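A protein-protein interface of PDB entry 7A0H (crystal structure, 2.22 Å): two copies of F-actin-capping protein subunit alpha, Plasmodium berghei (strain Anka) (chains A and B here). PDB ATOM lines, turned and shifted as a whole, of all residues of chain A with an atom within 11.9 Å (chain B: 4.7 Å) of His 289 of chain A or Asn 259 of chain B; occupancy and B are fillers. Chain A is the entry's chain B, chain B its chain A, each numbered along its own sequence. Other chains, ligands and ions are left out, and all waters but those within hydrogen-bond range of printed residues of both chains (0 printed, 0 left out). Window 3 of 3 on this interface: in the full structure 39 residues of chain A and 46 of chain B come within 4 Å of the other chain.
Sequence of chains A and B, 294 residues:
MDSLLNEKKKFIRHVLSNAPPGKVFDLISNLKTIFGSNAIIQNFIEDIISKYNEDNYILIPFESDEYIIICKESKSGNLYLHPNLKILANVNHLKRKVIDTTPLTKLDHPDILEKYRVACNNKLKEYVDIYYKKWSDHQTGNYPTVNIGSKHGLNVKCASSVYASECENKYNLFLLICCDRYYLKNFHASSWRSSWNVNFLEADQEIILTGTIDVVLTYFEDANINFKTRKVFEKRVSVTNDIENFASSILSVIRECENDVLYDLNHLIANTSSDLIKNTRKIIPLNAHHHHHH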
ATOM      1  N   ARG A 281      21.292 -17.728  19.083  1.00  0.00           N
ATOM      2  CA  ARG A 281      22.719 -17.522  19.362  1.00  0.00           C
ATOM      3  C   ARG A 281      23.485 -17.287  18.081  1.00  0.00           C
ATOM      4  O   ARG A 281      24.446 -16.524  18.086  1.00  0.00           O
ATOM      5  CB  ARG A 281      23.390 -18.699  20.086  1.00  0.00           C
ATOM      6  CG  ARG A 281      22.811 -19.075  21.424  1.00  0.00           C
ATOM      7  CD  ARG A 281      23.481 -20.402  21.924  1.00  0.00           C
ATOM      8  NE  ARG A 281      22.931 -20.753  23.228  1.00  0.00           N
ATOM      9  CZ  ARG A 281      23.027 -21.945  23.824  1.00  0.00           C
ATOM     10  NH1 ARG A 281      23.642 -22.964  23.228  1.00  0.00           N
ATOM     11  NH2 ARG A 281      22.491 -22.103  25.027  1.00  0.00           N
ATOM     12  N   ILE A 283      22.521 -15.301  15.927  1.00  0.00           N
ATOM     13  CA  ILE A 283      22.438 -13.898  15.619  1.00  0.00           C
ATOM     14  C   ILE A 283      23.643 -13.110  16.115  1.00  0.00           C
ATOM     15  O   ILE A 283      23.905 -11.987  15.602  1.00  0.00           O
ATOM     16  CB  ILE A 283      21.156 -13.358  16.269  1.00  0.00           C
ATOM     17  CG1 ILE A 283      19.917 -14.022  15.645  1.00  0.00           C
ATOM     18  CG2 ILE A 283      21.083 -11.855  16.144  1.00  0.00           C
ATOM     19  CD1 ILE A 283      18.712 -13.627  16.428  1.00  0.00           C
ATOM     20  N   ILE A 284      24.366 -13.620  17.120  1.00  0.00           N
ATOM     21  CA  ILE A 284      25.452 -12.816  17.710  1.00  0.00           C
ATOM     22  C   ILE A 284      26.436 -12.559  16.571  1.00  0.00           C
ATOM     23  O   ILE A 284      26.917 -13.515  15.930  1.00  0.00           O
ATOM     24  CB  ILE A 284      26.093 -13.523  18.897  1.00  0.00           C
ATOM     25  CG1 ILE A 284      25.037 -13.967  19.937  1.00  0.00           C
ATOM     26  CG2 ILE A 284      27.034 -12.592  19.542  1.00  0.00           C
ATOM     27  CD1 ILE A 284      24.803 -12.968  21.151  1.00  0.00           C
ATOM     28  N   PRO A 285      26.744 -11.307  16.244  1.00  0.00           N
ATOM     29  CA  PRO A 285      27.677 -11.063  15.115  1.00  0.00           C
ATOM     30  C   PRO A 285      29.162 -11.140  15.473  1.00  0.00           C
ATOM     31  O   PRO A 285      30.009 -11.182  14.556  1.00  0.00           O
ATOM     32  CB  PRO A 285      27.308  -9.651  14.661  1.00  0.00           C
ATOM     33  CG  PRO A 285      26.958  -9.010  16.023  1.00  0.00           C
ATOM     34  CD  PRO A 285      26.263 -10.058  16.870  1.00  0.00           C
ATOM     35  N   LEU A 286      29.505 -11.344  16.747  1.00  0.00           N
ATOM     36  CA  LEU A 286      30.911 -11.546  17.145  1.00  0.00           C
ATOM     37  C   LEU A 286      31.408 -12.933  16.818  1.00  0.00           C
ATOM     38  O   LEU A 286      30.698 -13.907  16.993  1.00  0.00           O
ATOM     39  CB  LEU A 286      31.005 -11.389  18.665  1.00  0.00           C
ATOM     40  CG  LEU A 286      30.460 -10.122  19.319  1.00  0.00           C
ATOM     41  CD1 LEU A 286      30.308 -10.313  20.776  1.00  0.00           C
ATOM     42  CD2 LEU A 286      31.366  -8.998  19.049  1.00  0.00           C
ATOM     43  N   ASN A 287      32.631 -13.036  16.293  1.00  0.00           N
ATOM     44  CA  ASN A 287      33.342 -14.326  16.341  1.00  0.00           C
ATOM     45  C   ASN A 287      33.421 -14.847  17.786  1.00  0.00           C
ATOM     46  O   ASN A 287      33.566 -14.066  18.731  1.00  0.00           O
ATOM     47  CB  ASN A 287      34.752 -14.173  15.804  1.00  0.00           C
ATOM     48  CG  ASN A 287      34.769 -13.999  14.339  1.00  0.00           C
ATOM     49  OD1 ASN A 287      34.270 -14.857  13.596  1.00  0.00           O
ATOM     50  ND2 ASN A 287      35.324 -12.878  13.888  1.00  0.00           N
ATOM     51  N   ALA A 288      33.405 -16.179  17.944  1.00  0.00           N
ATOM     52  CA  ALA A 288      32.868 -16.822  19.150  1.00  0.00           C
ATOM     53  C   ALA A 288      33.912 -17.172  20.228  1.00  0.00           C
ATOM     54  O   ALA A 288      33.597 -17.970  21.127  1.00  0.00           O
ATOM     55  CB  ALA A 288      32.127 -18.119  18.775  1.00  0.00           C
ATOM     56  N   HIS A 289      35.111 -16.587  20.186  1.00  0.00           N
ATOM     57  CA  HIS A 289      36.219 -17.017  21.053  1.00  0.00           C
ATOM     58  C   HIS A 289      36.507 -18.495  20.776  1.00  0.00           C
ATOM     59  O   HIS A 289      37.168 -18.839  19.795  1.00  0.00           O
ATOM     60  CB  HIS A 289      35.920 -16.811  22.554  1.00  0.00           C
ATOM     61  CG  HIS A 289      35.358 -15.456  22.891  1.00  0.00           C
ATOM     62  ND1 HIS A 289      36.143 -14.327  23.011  1.00  0.00           N
ATOM     63  CD2 HIS A 289      34.088 -15.056  23.153  1.00  0.00           C
ATOM     64  CE1 HIS A 289      35.380 -13.290  23.314  1.00  0.00           C
ATOM     65  NE2 HIS A 289      34.127 -13.703  23.397  1.00  0.00           N
ATOM     66  N   ARG B 255      32.794  -3.184  23.702  1.00  0.00           N
ATOM     67  CA  ARG B 255      33.367  -4.516  23.460  1.00  0.00           C
ATOM     68  C   ARG B 255      32.954  -5.500  24.564  1.00  0.00           C
ATOM     69  O   ARG B 255      32.517  -6.629  24.302  1.00  0.00           O
ATOM     70  CB  ARG B 255      34.905  -4.421  23.342  1.00  0.00           C
ATOM     71  CG  ARG B 255      35.637  -5.788  23.292  1.00  0.00           C
ATOM     72  CD  ARG B 255      37.156  -5.651  22.985  1.00  0.00           C
ATOM     73  NE  ARG B 255      37.808  -4.741  23.943  1.00  0.00           N
ATOM     74  CZ  ARG B 255      38.933  -4.102  23.702  1.00  0.00           C
ATOM     75  NH1 ARG B 255      39.578  -4.309  22.530  1.00  0.00           N
ATOM     76  NH2 ARG B 255      39.395  -3.279  24.630  1.00  0.00           N
ATOM     77  N   GLU B 256      32.984  -5.041  25.804  1.00  0.00           N
ATOM     78  CA  GLU B 256      32.673  -5.910  26.931  1.00  0.00           C
ATOM     79  C   GLU B 256      31.183  -6.172  27.048  1.00  0.00           C
ATOM     80  O   GLU B 256      30.754  -7.286  27.403  1.00  0.00           O
ATOM     81  CB  GLU B 256      33.170  -5.218  28.206  1.00  0.00           C
ATOM     82  CG  GLU B 256      33.192  -6.077  29.428  1.00  0.00           C
ATOM     83  CD  GLU B 256      33.124  -5.271  30.735  1.00  0.00           C
ATOM     84  OE1 GLU B 256      32.962  -4.017  30.680  1.00  0.00           O
ATOM     85  OE2 GLU B 256      33.170  -5.919  31.820  1.00  0.00           O
ATOM     86  N   CYS B 257      30.376  -5.131  26.908  1.00  0.00           N
ATOM     87  CA  CYS B 257      28.913  -5.356  26.964  1.00  0.00           C
ATOM     88  C   CYS B 257      28.433  -6.304  25.859  1.00  0.00           C
ATOM     89  O   CYS B 257      27.588  -7.183  26.106  1.00  0.00           O
ATOM     90  CB  CYS B 257      28.243  -3.999  26.929  1.00  0.00           C
ATOM     91  SG  CYS B 257      28.573  -3.036  28.464  1.00  0.00           S
ATOM     92  N   GLU B 258      29.056  -6.280  24.688  1.00  0.00           N
ATOM     93  CA  GLU B 258      28.590  -7.181  23.636  1.00  0.00           C
ATOM     94  C   GLU B 258      29.028  -8.591  23.952  1.00  0.00           C
ATOM     95  O   GLU B 258      28.294  -9.556  23.714  1.00  0.00           O
ATOM     96  CB  GLU B 258      29.079  -6.688  22.275  1.00  0.00           C
ATOM     97  CG  GLU B 258      28.325  -5.271  21.832  1.00  0.00           C
ATOM     98  CD  GLU B 258      28.437  -4.949  20.355  1.00  0.00           C
ATOM     99  OE1 GLU B 258      29.280  -5.545  19.688  1.00  0.00           O
ATOM    100  OE2 GLU B 258      27.751  -4.075  19.853  1.00  0.00           O
ATOM    101  N   ASN B 259      30.220  -8.718  24.532  1.00  0.00           N
ATOM    102  CA  ASN B 259      30.669 -10.012  25.052  1.00  0.00           C
ATOM    103  C   ASN B 259      29.710 -10.533  26.118  1.00  0.00           C
ATOM    104  O   ASN B 259      29.466 -11.727  26.202  1.00  0.00           O
ATOM    105  CB  ASN B 259      32.087  -9.867  25.709  1.00  0.00           C
ATOM    106  CG  ASN B 259      33.227  -9.982  24.701  1.00  0.00           C
ATOM    107  OD1 ASN B 259      33.111 -10.738  23.735  1.00  0.00           O
ATOM    108  ND2 ASN B 259      34.355  -9.240  24.940  1.00  0.00           N
ATOM    109  N   ASP B 260      29.189  -9.653  26.968  1.00  0.00           N
ATOM    110  CA  ASP B 260      28.289 -10.098  28.041  1.00  0.00           C
ATOM    111  C   ASP B 260      26.969 -10.642  27.473  1.00  0.00           C
ATOM    112  O   ASP B 260      26.413 -11.607  28.018  1.00  0.00           O
ATOM    113  CB  ASP B 260      28.110  -8.922  29.022  1.00  0.00           C
ATOM    114  CG  ASP B 260      27.214  -9.257  30.249  1.00  0.00           C
ATOM    115  OD1 ASP B 260      27.306 -10.374  30.848  1.00  0.00           O
ATOM    116  OD2 ASP B 260      26.428  -8.337  30.649  1.00  0.00           O
ATOM    117  N   VAL B 261      26.468 -10.074  26.354  1.00  0.00           N
ATOM    118  CA  VAL B 261      25.241 -10.607  25.729  1.00  0.00           C
ATOM    119  C   VAL B 261      25.536 -11.964  25.096  1.00  0.00           C
ATOM    120  O   VAL B 261      24.761 -12.927  25.224  1.00  0.00           O
ATOM    121  CB  VAL B 261      24.681  -9.609  24.676  1.00  0.00           C
ATOM    122  CG1 VAL B 261      23.581 -10.276  23.809  1.00  0.00           C
ATOM    123  CG2 VAL B 261      24.136  -8.341  25.331  1.00  0.00           C
ATOM    124  N   LEU B 262      26.682 -12.067  24.430  1.00  0.00           N
ATOM    125  CA  LEU B 262      27.095 -13.345  23.869  1.00  0.00           C
ATOM    126  C   LEU B 262      27.099 -14.395  24.942  1.00  0.00           C
ATOM    127  O   LEU B 262      26.598 -15.508  24.760  1.00  0.00           O
ATOM    128  CB  LEU B 262      28.482 -13.215  23.282  1.00  0.00           C
ATOM    129  CG  LEU B 262      28.966 -14.354  22.419  1.00  0.00           C
ATOM    130  CD1 LEU B 262      30.232 -13.958  21.674  1.00  0.00           C
ATOM    131  CD2 LEU B 262      29.227 -15.535  23.289  1.00  0.00           C
ATOM    132  N   TYR B 263      27.607 -14.041  26.096  1.00  0.00           N
ATOM    133  CA  TYR B 263      27.636 -15.004  27.176  1.00  0.00           C
ATOM    134  C   TYR B 263      26.221 -15.342  27.607  1.00  0.00           C
ATOM    135  O   TYR B 263      25.911 -16.507  27.831  1.00  0.00           O
ATOM    136  CB  TYR B 263      28.440 -14.437  28.329  1.00  0.00           C
ATOM    137  CG  TYR B 263      28.351 -15.319  29.531  1.00  0.00           C
ATOM    138  CD1 TYR B 263      29.287 -16.318  29.775  1.00  0.00           C
ATOM    139  CD2 TYR B 263      27.303 -15.153  30.436  1.00  0.00           C
ATOM    140  CE1 TYR B 263      29.185 -17.116  30.922  1.00  0.00           C
ATOM    141  CE2 TYR B 263      27.173 -15.941  31.549  1.00  0.00           C
ATOM    142  CZ  TYR B 263      28.109 -16.937  31.794  1.00  0.00           C
ATOM    143  OH  TYR B 263      27.937 -17.710  32.914  1.00  0.00           O
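No position is printed for both chains. Of the 5 pairs that touch across the chains among the printed residues, none has its exchanged pair printed and touching as well.
A ring nitrogen (NE2) of His 289 of chain A is in hydrogen-bond range of the side-chain amide oxygen of Asn 259 of chain B (3.2 Å).
Of the 9 printed residues of chain B, 4 touch a printed residue of chain A. Along chain B the printed residues that touch a printed residue of chain A span positions 258 to 262. Of the 8 printed residues of chain A, 3 touch a printed residue of chain B. Hydrophobic or aromatic side chains of chain A within 4 Å of the printed part of chain B: Ile 284, Leu 286 and His 289. Along chain A the printed residues that touch a printed residue of chain B span positions 284 to 289. Among the printed residues, 5 pairs touch across the chains. Among the printed residues, no Asp or Glu carboxylate lies within 4 Å of a Lys or Arg side-chain nitrogen of the other chain.
The backbone carbonyl oxygen of Arg 255 of chain B lies within hydrogen-bond range of the side-chain amide nitrogen of Asn 259 of chain B (3.3 Å).
Printed residues of chain B within 4 Å of Ile 284 of chain A: Val 261 and Leu 262. Of the printed residues of chain B, Leu 286 of chain A touches Glu 258 and Leu 262. His 289 of chain A touches one residue of chain B. No residue of chain A comes within 4 Å of Arg 255 of chain B. No residue of chain A comes within 4 Å of Glu 256 of chain B. No residue of chain A comes within 4 Å of Cys 257 of chain B. Printed residues of chain A within 4 Å of Glu 258 of chain B: Leu 286 (3.6 Å). Asn 259 of chain B touches just one residue of chain A: His 289. Of chain A, only Ile 284 comes within 4 Å of Val 261 of chain B. Leu 262 of chain B touches just these residues of chain A: Ile 284 and Leu 286. Tyr 263 of chain B touches none of the printed residues of chain A. The nearest residue of chain B that does not touch His 289 of chain A is Leu 262 of chain B (4.3 Å).
Val 261 of chain B touches Ile 284 of chain A (CG1 to CD1, 3.98 Å). CD1 of Ile 284 of chain A touches CA of Leu 262 of chain B, at 3.6 Å. Glu 258 of chain B touches Leu 286 of chain A. Leu 286 of chain A touches Leu 262 of chain B.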
